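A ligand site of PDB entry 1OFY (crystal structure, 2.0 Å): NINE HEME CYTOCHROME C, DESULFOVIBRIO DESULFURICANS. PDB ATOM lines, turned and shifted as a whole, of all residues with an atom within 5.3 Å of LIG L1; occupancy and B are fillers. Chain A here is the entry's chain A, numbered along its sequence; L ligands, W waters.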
ATOM      1  N   SER A   8      14.354 -25.069  11.578  1.00  0.00           N
ATOM      2  CA  SER A   8      13.895 -26.415  11.296  1.00  0.00           C
ATOM      3  C   SER A   8      14.863 -27.511  11.709  1.00  0.00           C
ATOM      4  O   SER A   8      14.453 -28.664  11.896  1.00  0.00           O
ATOM      5  CB  SER A   8      13.608 -26.575   9.784  1.00  0.00           C
ATOM      6  OG  SER A   8      14.845 -26.532   9.087  1.00  0.00           O
ATOM      7  N   GLY A   9      16.144 -27.230  11.838  1.00  0.00           N
ATOM      8  CA  GLY A   9      17.073 -28.322  12.103  1.00  0.00           C
ATOM      9  C   GLY A   9      17.642 -28.926  10.835  1.00  0.00           C
ATOM     10  O   GLY A   9      18.602 -29.712  10.875  1.00  0.00           O
ATOM     11  N   ALA A  10      17.084 -28.606   9.666  1.00  0.00           N
ATOM     12  CA  ALA A  10      17.753 -29.046   8.439  1.00  0.00           C
ATOM     13  C   ALA A  10      19.032 -28.239   8.278  1.00  0.00           C
ATOM     14  O   ALA A  10      19.227 -27.164   8.868  1.00  0.00           O
ATOM     15  CB  ALA A  10      16.862 -28.905   7.227  1.00  0.00           C
ATOM     16  N   PRO A  11      19.972 -28.733   7.493  1.00  0.00           N
ATOM     17  CA  PRO A  11      21.229 -27.960   7.352  1.00  0.00           C
ATOM     18  C   PRO A  11      20.904 -26.646   6.662  1.00  0.00           C
ATOM     19  O   PRO A  11      19.927 -26.574   5.903  1.00  0.00           O
ATOM     20  CB  PRO A  11      22.090 -28.875   6.491  1.00  0.00           C
ATOM     21  CG  PRO A  11      21.454 -30.231   6.582  1.00  0.00           C
ATOM     22  CD  PRO A  11      19.980 -29.968   6.694  1.00  0.00           C
ATOM     23  N   ILE A  14      22.716 -27.229   1.559  1.00  0.00           N
ATOM     24  CA  ILE A  14      22.917 -28.644   1.317  1.00  0.00           C
ATOM     25  C   ILE A  14      23.346 -28.984  -0.104  1.00  0.00           C
ATOM     26  O   ILE A  14      22.671 -28.609  -1.057  1.00  0.00           O
ATOM     27  CB  ILE A  14      21.583 -29.389   1.557  1.00  0.00           C
ATOM     28  CG1 ILE A  14      20.811 -28.923   2.781  1.00  0.00           C
ATOM     29  CG2 ILE A  14      21.823 -30.891   1.614  1.00  0.00           C
ATOM     30  CD1 ILE A  14      19.375 -29.405   2.851  1.00  0.00           C
ATOM     31  N   VAL A  15      24.431 -29.741  -0.257  1.00  0.00           N
ATOM     32  CA  VAL A  15      24.721 -30.272  -1.595  1.00  0.00           C
ATOM     33  C   VAL A  15      23.816 -31.449  -1.933  1.00  0.00           C
ATOM     34  O   VAL A  15      23.756 -32.443  -1.205  1.00  0.00           O
ATOM     35  CB  VAL A  15      26.200 -30.696  -1.701  1.00  0.00           C
ATOM     36  CG1 VAL A  15      26.581 -31.033  -3.138  1.00  0.00           C
ATOM     37  CG2 VAL A  15      27.097 -29.580  -1.158  1.00  0.00           C
ATOM     38  N   MET A  16      23.091 -31.386  -3.054  1.00  0.00           N
ATOM     39  CA  MET A  16      22.266 -32.477  -3.534  1.00  0.00           C
ATOM     40  C   MET A  16      23.006 -33.210  -4.659  1.00  0.00           C
ATOM     41  O   MET A  16      23.515 -32.549  -5.578  1.00  0.00           O
ATOM     42  CB  MET A  16      20.896 -31.998  -3.998  1.00  0.00           C
ATOM     43  CG  MET A  16      20.177 -31.181  -2.908  1.00  0.00           C
ATOM     44  SD  MET A  16      18.626 -30.456  -3.442  1.00  0.00           S
ATOM     45  CE  MET A  16      17.588 -31.840  -3.856  1.00  0.00           C
ATOM     46  N   PHE A  35      21.362 -26.478  -2.441  1.00  0.00           N
ATOM     47  CA  PHE A  35      20.059 -25.918  -2.086  1.00  0.00           C
ATOM     48  C   PHE A  35      20.134 -25.124  -0.797  1.00  0.00           C
ATOM     49  O   PHE A  35      20.589 -25.619   0.237  1.00  0.00           O
ATOM     50  CB  PHE A  35      19.040 -27.048  -1.975  1.00  0.00           C
ATOM     51  CG  PHE A  35      17.647 -26.666  -1.531  1.00  0.00           C
ATOM     52  CD1 PHE A  35      16.802 -25.955  -2.372  1.00  0.00           C
ATOM     53  CD2 PHE A  35      17.178 -27.028  -0.279  1.00  0.00           C
ATOM     54  CE1 PHE A  35      15.524 -25.633  -1.962  1.00  0.00           C
ATOM     55  CE2 PHE A  35      15.891 -26.695   0.129  1.00  0.00           C
ATOM     56  CZ  PHE A  35      15.045 -25.985  -0.711  1.00  0.00           C
ATOM     57  N   HIS A  37      18.456 -24.191   2.138  1.00  0.00           N
ATOM     58  CA  HIS A  37      17.287 -24.552   2.916  1.00  0.00           C
ATOM     59  C   HIS A  37      16.851 -23.355   3.762  1.00  0.00           C
ATOM     60  O   HIS A  37      15.665 -23.096   3.922  1.00  0.00           O
ATOM     61  CB  HIS A  37      17.536 -25.790   3.800  1.00  0.00           C
ATOM     62  CG  HIS A  37      16.289 -26.585   4.078  1.00  0.00           C
ATOM     63  ND1 HIS A  37      15.383 -26.151   5.034  1.00  0.00           N
ATOM     64  CD2 HIS A  37      15.758 -27.719   3.565  1.00  0.00           C
ATOM     65  CE1 HIS A  37      14.385 -27.009   5.072  1.00  0.00           C
ATOM     66  NE2 HIS A  37      14.563 -27.981   4.195  1.00  0.00           N
ATOM     67  N   HIS A  40      14.802 -20.840   1.795  1.00  0.00           N
ATOM     68  CA  HIS A  40      13.510 -21.353   1.367  1.00  0.00           C
ATOM     69  C   HIS A  40      12.556 -21.544   2.544  1.00  0.00           C
ATOM     70  O   HIS A  40      11.344 -21.313   2.430  1.00  0.00           O
ATOM     71  CB  HIS A  40      13.651 -22.667   0.600  1.00  0.00           C
ATOM     72  CG  HIS A  40      14.105 -22.507  -0.829  1.00  0.00           C
ATOM     73  ND1 HIS A  40      15.430 -22.332  -1.154  1.00  0.00           N
ATOM     74  CD2 HIS A  40      13.442 -22.515  -2.002  1.00  0.00           C
ATOM     75  CE1 HIS A  40      15.554 -22.226  -2.460  1.00  0.00           C
ATOM     76  NE2 HIS A  40      14.353 -22.336  -3.011  1.00  0.00           N
ATOM     77  N   GLU A  41      13.070 -21.985   3.706  1.00  0.00           N
ATOM     78  CA  GLU A  41      12.149 -22.293   4.811  1.00  0.00           C
ATOM     79  C   GLU A  41      11.629 -20.990   5.406  1.00  0.00           C
ATOM     80  O   GLU A  41      10.512 -20.926   5.902  1.00  0.00           O
ATOM     81  CB  GLU A  41      12.784 -23.182   5.863  1.00  0.00           C
ATOM     82  CG  GLU A  41      13.873 -22.553   6.717  1.00  0.00           C
ATOM     83  CD  GLU A  41      14.398 -23.545   7.747  1.00  0.00           C
ATOM     84  OE1 GLU A  41      15.012 -24.553   7.333  1.00  0.00           O
ATOM     85  OE2 GLU A  41      14.202 -23.321   8.955  1.00  0.00           O
ATOM     86  N   ILE A  44       8.793 -19.990   2.560  1.00  0.00           N
ATOM     87  CA  ILE A  44       7.654 -20.890   2.351  1.00  0.00           C
ATOM     88  C   ILE A  44       7.197 -21.436   3.707  1.00  0.00           C
ATOM     89  O   ILE A  44       7.939 -22.108   4.412  1.00  0.00           O
ATOM     90  CB  ILE A  44       7.986 -22.047   1.393  1.00  0.00           C
ATOM     91  CG1 ILE A  44       8.799 -21.668   0.149  1.00  0.00           C
ATOM     92  CG2 ILE A  44       6.720 -22.800   0.995  1.00  0.00           C
ATOM     93  CD1 ILE A  44       8.042 -20.866  -0.880  1.00  0.00           C
ATOM     94  N   ASN A  46       4.657 -23.633   4.878  1.00  0.00           N
ATOM     95  CA  ASN A  46       4.408 -25.029   5.231  1.00  0.00           C
ATOM     96  C   ASN A  46       5.540 -25.943   4.768  1.00  0.00           C
ATOM     97  O   ASN A  46       5.824 -26.038   3.565  1.00  0.00           O
ATOM     98  CB  ASN A  46       3.064 -25.468   4.633  1.00  0.00           C
ATOM     99  CG  ASN A  46       2.666 -26.869   5.064  1.00  0.00           C
ATOM    100  OD1 ASN A  46       3.265 -27.466   5.960  1.00  0.00           O
ATOM    101  ND2 ASN A  46       1.630 -27.398   4.416  1.00  0.00           N
ATOM    102  N   CYS A  47       6.177 -26.629   5.711  1.00  0.00           N
ATOM    103  CA  CYS A  47       7.195 -27.615   5.411  1.00  0.00           C
ATOM    104  C   CYS A  47       6.695 -28.597   4.346  1.00  0.00           C
ATOM    105  O   CYS A  47       7.440 -29.039   3.464  1.00  0.00           O
ATOM    106  CB  CYS A  47       7.601 -28.452   6.611  1.00  0.00           C
ATOM    107  SG  CYS A  47       8.204 -27.666   8.109  1.00  0.00           S
ATOM    108  N   THR A  49       4.557 -28.362   2.053  1.00  0.00           N
ATOM    109  CA  THR A  49       4.491 -27.879   0.680  1.00  0.00           C
ATOM    110  C   THR A  49       5.517 -28.647  -0.161  1.00  0.00           C
ATOM    111  O   THR A  49       5.287 -29.219  -1.214  1.00  0.00           O
ATOM    112  CB  THR A  49       4.785 -26.378   0.595  1.00  0.00           C
ATOM    113  OG1 THR A  49       3.728 -25.657   1.226  1.00  0.00           O
ATOM    114  CG2 THR A  49       4.836 -25.933  -0.852  1.00  0.00           C
ATOM    115  N   CYS A  50       6.747 -28.677   0.356  1.00  0.00           N
ATOM    116  CA  CYS A  50       7.813 -29.386  -0.350  1.00  0.00           C
ATOM    117  C   CYS A  50       7.870 -30.844   0.053  1.00  0.00           C
ATOM    118  O   CYS A  50       7.822 -31.739  -0.808  1.00  0.00           O
ATOM    119  CB  CYS A  50       9.135 -28.669  -0.046  1.00  0.00           C
ATOM    120  SG  CYS A  50       9.042 -26.935  -0.595  1.00  0.00           S
ATOM    121  N   HIS A  51       7.961 -31.058   1.367  1.00  0.00           N
ATOM    122  CA  HIS A  51       7.979 -32.436   1.880  1.00  0.00           C
ATOM    123  C   HIS A  51       6.544 -32.961   1.862  1.00  0.00           C
ATOM    124  O   HIS A  51       5.907 -33.046   2.905  1.00  0.00           O
ATOM    125  CB  HIS A  51       8.615 -32.484   3.266  1.00  0.00           C
ATOM    126  CG  HIS A  51       9.961 -31.828   3.340  1.00  0.00           C
ATOM    127  ND1 HIS A  51      11.131 -32.463   2.969  1.00  0.00           N
ATOM    128  CD2 HIS A  51      10.354 -30.594   3.760  1.00  0.00           C
ATOM    129  CE1 HIS A  51      12.160 -31.649   3.145  1.00  0.00           C
ATOM    130  NE2 HIS A  51      11.725 -30.501   3.627  1.00  0.00           N
ATOM    131  N   PRO A  56      10.057 -35.397   6.741  1.00  0.00           N
ATOM    132  CA  PRO A  56      11.060 -34.328   6.626  1.00  0.00           C
ATOM    133  C   PRO A  56      12.366 -34.978   6.220  1.00  0.00           C
ATOM    134  O   PRO A  56      13.321 -35.058   6.983  1.00  0.00           O
ATOM    135  CB  PRO A  56      11.136 -33.795   8.045  1.00  0.00           C
ATOM    136  CG  PRO A  56      10.922 -35.025   8.878  1.00  0.00           C
ATOM    137  CD  PRO A  56       9.857 -35.807   8.142  1.00  0.00           C
ATOM    138  N   VAL A  57      12.403 -35.502   4.993  1.00  0.00           N
ATOM    139  CA  VAL A  57      13.578 -36.265   4.607  1.00  0.00           C
ATOM    140  C   VAL A  57      14.005 -35.923   3.185  1.00  0.00           C
ATOM    141  O   VAL A  57      13.225 -35.410   2.392  1.00  0.00           O
ATOM    142  CB  VAL A  57      13.301 -37.776   4.714  1.00  0.00           C
ATOM    143  CG1 VAL A  57      13.031 -38.200   6.145  1.00  0.00           C
ATOM    144  CG2 VAL A  57      12.128 -38.159   3.818  1.00  0.00           C
ATOM    145  N   SER A  58      15.259 -36.211   2.868  1.00  0.00           N
ATOM    146  CA  SER A  58      15.783 -35.957   1.539  1.00  0.00           C
ATOM    147  C   SER A  58      14.915 -36.551   0.452  1.00  0.00           C
ATOM    148  O   SER A  58      14.543 -37.718   0.540  1.00  0.00           O
ATOM    149  CB  SER A  58      17.199 -36.531   1.453  1.00  0.00           C
ATOM    150  OG  SER A  58      18.016 -35.776   2.342  1.00  0.00           O
ATOM    151  N   CYS A  59      14.564 -35.762  -0.556  1.00  0.00           N
ATOM    152  CA  CYS A  59      13.765 -36.267  -1.667  1.00  0.00           C
ATOM    153  C   CYS A  59      14.367 -37.543  -2.232  1.00  0.00           C
ATOM    154  O   CYS A  59      13.655 -38.483  -2.594  1.00  0.00           O
ATOM    155  CB  CYS A  59      13.632 -35.242  -2.813  1.00  0.00           C
ATOM    156  SG  CYS A  59      13.374 -33.538  -2.259  1.00  0.00           S
ATOM    157  N   SER A  60      15.700 -37.576  -2.322  1.00  0.00           N
ATOM    158  CA  SER A  60      16.345 -38.691  -3.005  1.00  0.00           C
ATOM    159  C   SER A  60      16.166 -39.996  -2.234  1.00  0.00           C
ATOM    160  O   SER A  60      16.489 -41.055  -2.789  1.00  0.00           O
ATOM    161  CB  SER A  60      17.831 -38.433  -3.207  1.00  0.00           C
ATOM    162  OG  SER A  60      18.412 -37.893  -2.033  1.00  0.00           O
HETATM  163 FE1  LIG L   1      13.203 -29.321   3.890  1.00  0.00          FE
HETATM  164  C1  LIG L   1      15.762 -31.401   3.145  1.00  0.00           C
HETATM  165  C2  LIG L   1      13.075 -30.523   7.000  1.00  0.00           C
HETATM  166  C3  LIG L   1      10.899 -26.935   4.706  1.00  0.00           C
HETATM  167  C4  LIG L   1      12.937 -28.456   0.611  1.00  0.00           C
HETATM  168  N1  LIG L   1      14.416 -30.498   4.966  1.00  0.00           N
HETATM  169  C5  LIG L   1      15.337 -31.394   4.445  1.00  0.00           C
HETATM  170  C6  LIG L   1      15.762 -32.290   5.494  1.00  0.00           C
HETATM  171  C7  LIG L   1      15.140 -31.921   6.625  1.00  0.00           C
HETATM  172  C8  LIG L   1      14.139 -30.948   6.239  1.00  0.00           C
HETATM  173  C9  LIG L   1      15.385 -32.392   8.067  1.00  0.00           C
HETATM  174  C10 LIG L   1      16.744 -33.455   5.281  1.00  0.00           C
HETATM  175  C11 LIG L   1      18.191 -33.013   5.547  1.00  0.00           C
HETATM  176  C12 LIG L   1      19.210 -33.859   4.807  1.00  0.00           C
HETATM  177  O1  LIG L   1      18.863 -35.025   4.500  1.00  0.00           O
HETATM  178  O2  LIG L   1      20.305 -33.305   4.548  1.00  0.00           O
HETATM  179  N2  LIG L   1      12.228 -28.780   5.566  1.00  0.00           N
HETATM  180  C13 LIG L   1      12.273 -29.429   6.783  1.00  0.00           C
HETATM  181  C14 LIG L   1      11.380 -28.783   7.720  1.00  0.00           C
HETATM  182  C15 LIG L   1      10.755 -27.802   7.064  1.00  0.00           C
HETATM  183  C16 LIG L   1      11.263 -27.805   5.718  1.00  0.00           C
HETATM  184  C17 LIG L   1      11.211 -29.172   9.193  1.00  0.00           C
HETATM  185  C18 LIG L   1       9.701 -26.816   7.572  1.00  0.00           C
HETATM  186  C19 LIG L   1      10.166 -25.994   8.775  1.00  0.00           C
HETATM  187  N3  LIG L   1      12.032 -28.082   2.859  1.00  0.00           N
HETATM  188  C20 LIG L   1      11.166 -27.134   3.372  1.00  0.00           C
HETATM  189  C21 LIG L   1      10.541 -26.397   2.303  1.00  0.00           C
HETATM  190  C22 LIG L   1      11.097 -26.840   1.161  1.00  0.00           C
HETATM  191  C23 LIG L   1      12.083 -27.844   1.496  1.00  0.00           C
HETATM  192  C24 LIG L   1       9.450 -25.347   2.474  1.00  0.00           C
HETATM  193  C25 LIG L   1      10.753 -26.422  -0.276  1.00  0.00           C
HETATM  194  C26 LIG L   1      10.849 -24.925  -0.550  1.00  0.00           C
HETATM  195  N4  LIG L   1      14.166 -29.809   2.203  1.00  0.00           N
HETATM  196  C27 LIG L   1      13.884 -29.404   0.920  1.00  0.00           C
HETATM  197  C28 LIG L   1      14.715 -30.103  -0.029  1.00  0.00           C
HETATM  198  C29 LIG L   1      15.405 -31.023   0.672  1.00  0.00           C
HETATM  199  C30 LIG L   1      15.143 -30.770   2.074  1.00  0.00           C
HETATM  200  C31 LIG L   1      14.766 -29.807  -1.527  1.00  0.00           C
HETATM  201  C32 LIG L   1      16.286 -32.171   0.158  1.00  0.00           C
HETATM  202  C33 LIG L   1      17.795 -31.851   0.287  1.00  0.00           C
HETATM  203  C34 LIG L   1      18.666 -33.091   0.214  1.00  0.00           C
HETATM  204  O3  LIG L   1      18.469 -33.926  -0.710  1.00  0.00           O
HETATM  205  O4  LIG L   1      19.527 -33.205   1.107  1.00  0.00           O
HETATM  206 FE1  LG2 L   2      13.703 -22.261  -4.888  1.00  0.00          FE
HETATM  207  C1  LG2 L   2      14.917 -19.103  -4.409  1.00  0.00           C
HETATM  208  C2  LG2 L   2      16.732 -23.290  -5.980  1.00  0.00           C
HETATM  209  C3  LG2 L   2      12.634 -25.521  -4.820  1.00  0.00           C
HETATM  210  C4  LG2 L   2      10.609 -21.219  -4.025  1.00  0.00           C
HETATM  211  N1  LG2 L   2      15.457 -21.367  -5.187  1.00  0.00           N
HETATM  212  C5  LG2 L   2      15.761 -20.045  -4.990  1.00  0.00           C
HETATM  213  C6  LG2 L   2      17.100 -19.776  -5.468  1.00  0.00           C
HETATM  214  C7  LG2 L   2      17.585 -20.931  -5.958  1.00  0.00           C
HETATM  215  C8  LG2 L   2      16.583 -21.949  -5.721  1.00  0.00           C
HETATM  216  C9  LG2 L   2      18.938 -21.195  -6.630  1.00  0.00           C
HETATM  217  C10 LG2 L   2      17.742 -18.391  -5.377  1.00  0.00           C
HETATM  218  C11 LG2 L   2      18.358 -18.156  -3.973  1.00  0.00           C
HETATM  219  C12 LG2 L   2      19.709 -18.834  -3.889  1.00  0.00           C
HETATM  220  O1  LG2 L   2      20.589 -18.458  -4.695  1.00  0.00           O
HETATM  221  O2  LG2 L   2      19.814 -19.741  -3.029  1.00  0.00           O
HETATM  222  N2  LG2 L   2      14.515 -24.036  -5.335  1.00  0.00           N
HETATM  223  C13 LG2 L   2      15.803 -24.269  -5.752  1.00  0.00           C
HETATM  224  C14 LG2 L   2      16.023 -25.694  -5.934  1.00  0.00           C
HETATM  225  C15 LG2 L   2      14.882 -26.305  -5.579  1.00  0.00           C
HETATM  226  C16 LG2 L   2      13.930 -25.279  -5.210  1.00  0.00           C
HETATM  227  C17 LG2 L   2      17.336 -26.277  -6.459  1.00  0.00           C
HETATM  228  C18 LG2 L   2      14.505 -27.780  -5.533  1.00  0.00           C
HETATM  229  C19 LG2 L   2      15.439 -28.693  -4.730  1.00  0.00           C
HETATM  230  N3  LG2 L   2      11.980 -23.189  -4.508  1.00  0.00           N
HETATM  231  C20 LG2 L   2      11.698 -24.539  -4.559  1.00  0.00           C
HETATM  232  C21 LG2 L   2      10.297 -24.770  -4.289  1.00  0.00           C
HETATM  233  C22 LG2 L   2       9.727 -23.562  -4.081  1.00  0.00           C
HETATM  234  C23 LG2 L   2      10.783 -22.570  -4.203  1.00  0.00           C
HETATM  235  C24 LG2 L   2       9.688 -26.172  -4.272  1.00  0.00           C
HETATM  236  C25 LG2 L   2       8.286 -23.139  -3.802  1.00  0.00           C
HETATM  237  C26 LG2 L   2       7.403 -24.135  -3.028  1.00  0.00           C
HETATM  238  N4  LG2 L   2      12.939 -20.518  -4.281  1.00  0.00           N
HETATM  239  C27 LG2 L   2      11.609 -20.275  -3.963  1.00  0.00           C
HETATM  240  C28 LG2 L   2      11.455 -18.900  -3.556  1.00  0.00           C
HETATM  241  C29 LG2 L   2      12.685 -18.344  -3.555  1.00  0.00           C
HETATM  242  C30 LG2 L   2      13.599 -19.323  -4.098  1.00  0.00           C
HETATM  243  C31 LG2 L   2      10.125 -18.251  -3.189  1.00  0.00           C
HETATM  244  C32 LG2 L   2      13.103 -16.947  -3.117  1.00  0.00           C
HETATM  245  C33 LG2 L   2      13.319 -16.809  -1.607  1.00  0.00           C
HETATM  246  C34 LG2 L   2      13.417 -15.358  -1.156  1.00  0.00           C
HETATM  247  O3  LG2 L   2      14.010 -15.113  -0.077  1.00  0.00           O
HETATM  248  O4  LG2 L   2      12.904 -14.483  -1.881  1.00  0.00           O
HETATM  249 FE1  LG3 L   3       7.950 -37.066  -4.073  1.00  0.00          FE
HETATM  250  C1  LG3 L   3       5.630 -37.758  -6.621  1.00  0.00           C
HETATM  251  C2  LG3 L   3       8.818 -34.256  -5.700  1.00  0.00           C
HETATM  252  C3  LG3 L   3      10.176 -36.288  -1.544  1.00  0.00           C
HETATM  253  C4  LG3 L   3       7.375 -39.996  -2.738  1.00  0.00           C
HETATM  254  N1  LG3 L   3       7.355 -36.236  -5.809  1.00  0.00           N
HETATM  255  C5  LG3 L   3       6.342 -36.576  -6.684  1.00  0.00           C
HETATM  256  C6  LG3 L   3       6.117 -35.527  -7.645  1.00  0.00           C
HETATM  257  C7  LG3 L   3       7.087 -34.613  -7.461  1.00  0.00           C
HETATM  258  C8  LG3 L   3       7.818 -35.009  -6.271  1.00  0.00           C
HETATM  259  C9  LG3 L   3       7.368 -33.366  -8.300  1.00  0.00           C
HETATM  260  C10 LG3 L   3       4.963 -35.500  -8.657  1.00  0.00           C
HETATM  261  C11 LG3 L   3       5.379 -36.157  -9.982  1.00  0.00           C
HETATM  262  C12 LG3 L   3       4.257 -36.169 -10.999  1.00  0.00           C
HETATM  263  O1  LG3 L   3       3.078 -36.115 -10.579  1.00  0.00           O
HETATM  264  O2  LG3 L   3       4.586 -36.210 -12.206  1.00  0.00           O
HETATM  265  N2  LG3 L   3       9.184 -35.558  -3.655  1.00  0.00           N
HETATM  266  C13 LG3 L   3       9.403 -34.452  -4.479  1.00  0.00           C
HETATM  267  C14 LG3 L   3      10.325 -33.546  -3.835  1.00  0.00           C
HETATM  268  C15 LG3 L   3      10.706 -34.116  -2.681  1.00  0.00           C
HETATM  269  C16 LG3 L   3      10.010 -35.379  -2.577  1.00  0.00           C
HETATM  270  C17 LG3 L   3      10.778 -32.201  -4.412  1.00  0.00           C
HETATM  271  C18 LG3 L   3      11.684 -33.604  -1.625  1.00  0.00           C
HETATM  272  C19 LG3 L   3      11.323 -32.232  -1.062  1.00  0.00           C
HETATM  273  N3  LG3 L   3       8.565 -37.913  -2.363  1.00  0.00           N
HETATM  274  C20 LG3 L   3       9.550 -37.511  -1.486  1.00  0.00           C
HETATM  275  C21 LG3 L   3       9.829 -38.562  -0.525  1.00  0.00           C
HETATM  276  C22 LG3 L   3       9.092 -39.627  -0.900  1.00  0.00           C
HETATM  277  C23 LG3 L   3       8.290 -39.233  -2.042  1.00  0.00           C
HETATM  278  C24 LG3 L   3      10.774 -38.359   0.657  1.00  0.00           C
HETATM  279  C25 LG3 L   3       9.101 -41.022  -0.245  1.00  0.00           C
HETATM  280  C26 LG3 L   3       8.836 -40.960   1.285  1.00  0.00           C
HETATM  281  N4  LG3 L   3       6.751 -38.560  -4.619  1.00  0.00           N
HETATM  282  C27 LG3 L   3       6.611 -39.692  -3.832  1.00  0.00           C
HETATM  283  C28 LG3 L   3       5.528 -40.495  -4.356  1.00  0.00           C
HETATM  284  C29 LG3 L   3       4.905 -39.772  -5.315  1.00  0.00           C
HETATM  285  C30 LG3 L   3       5.760 -38.649  -5.580  1.00  0.00           C
HETATM  286  C31 LG3 L   3       5.150 -41.909  -3.888  1.00  0.00           C
HETATM  287  C32 LG3 L   3       3.576 -40.061  -6.011  1.00  0.00           C
HETATM  288  C33 LG3 L   3       2.394 -39.417  -5.246  1.00  0.00           C
HETATM  289  C34 LG3 L   3       1.148 -39.249  -6.093  1.00  0.00           C
HETATM  290  O3  LG3 L   3       1.035 -39.936  -7.135  1.00  0.00           O
HETATM  291  O4  LG3 L   3       0.295 -38.416  -5.708  1.00  0.00           O
HETATM  292  O   HOH W   1      22.722 -34.157   4.164  1.00  0.00           O
HETATM  293  O   HOH W   2      21.973 -34.259   0.018  1.00  0.00           O
HETATM  294  O   HOH W   3       8.682 -24.008   6.004  1.00  0.00           O
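The side-chain carboxylate (OE1) of Glu 41 is in hydrogen-bond range of a ring nitrogen (ND1) of His 37 (2.8 Å). The backbone carbonyl oxygen of Ile 14 sits at hydrogen-bond distance from the backbone NH of Phe 35, 2.9 Å away. The backbone NH (N) of Ala 10 lies within hydrogen-bond range of the side-chain hydroxyl (OG) of Ser 8 (3.1 Å). The side-chain carboxylate of Glu 41 is in hydrogen-bond range of the side-chain hydroxyl of Ser 8 (2.6 Å). O of Asn 46 sits at hydrogen-bond distance from OG1 of Thr 49, at 3.2 Å.
SG of Cys 47 is covalently linked to C18 of LIG L1 (1.8 Å). SG of Cys 50 is covalently linked to C25 of LIG L1 (1.8 Å). An iron atom (FE1) of LIG L1 is bound by a ring nitrogen (NE2) of His 51. FE1 of LIG L1 is bound by NE2 of His 37 (1.9 Å). The side-chain hydroxyl (OG) of Ser 58 sits at hydrogen-bond distance from an oxygen (O1) of LIG L1, 2.4 Å away. An iron atom (FE1) of LG2 L2 is bound by a ring nitrogen (NE2) of His 40, at 2.0 Å. A carbon (C18) of LG3 L3 is covalently linked to the side-chain sulfur (SG) of Cys 59, at 1.8 Å.
CB of Ser 8 touches C17 of LIG L1, 3.6 Å away. CB of Ala 10 touches C7 of LIG L1 (3.5 Å). Pro 11 touches LIG L1. CG2 of Ile 14 touches O4 of LIG L1, 3.3 Å away. Met 16 touches LIG L1 (CE to O3, 3.9 Å). CE2 of Phe 35 touches C27 of LIG L1, 3.5 Å away. His 40 touches LIG L1 (CB to C26, 3.8 Å). Ile 44 touches LIG L1 (CB to C24, 3.8 Å). Asn 46 touches LIG L1. O of Pro 56 touches C9 of LIG L1, 3.5 Å away. Hydrophobic or aromatic side chains within 4 Å of LIG L1: Ala 10, Pro 11, Ile 14, Met 16, Phe 35, His 37, His 40, Ile 44, His 51 and Pro 56. 15 residues have an atom within 4 Å of LIG L1: Ser 8, Ala 10, Pro 11, Ile 14, Met 16, Phe 35, His 37, His 40, Ile 44, Asn 46, Cys 47, Cys 50, His 51, Pro 56 and Ser 58.
Water W2 bridges the backbone carbonyl oxygen (O) of Val 15 (2.8 Å) and an oxygen (O4) of LIG L1 (2.9 Å).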
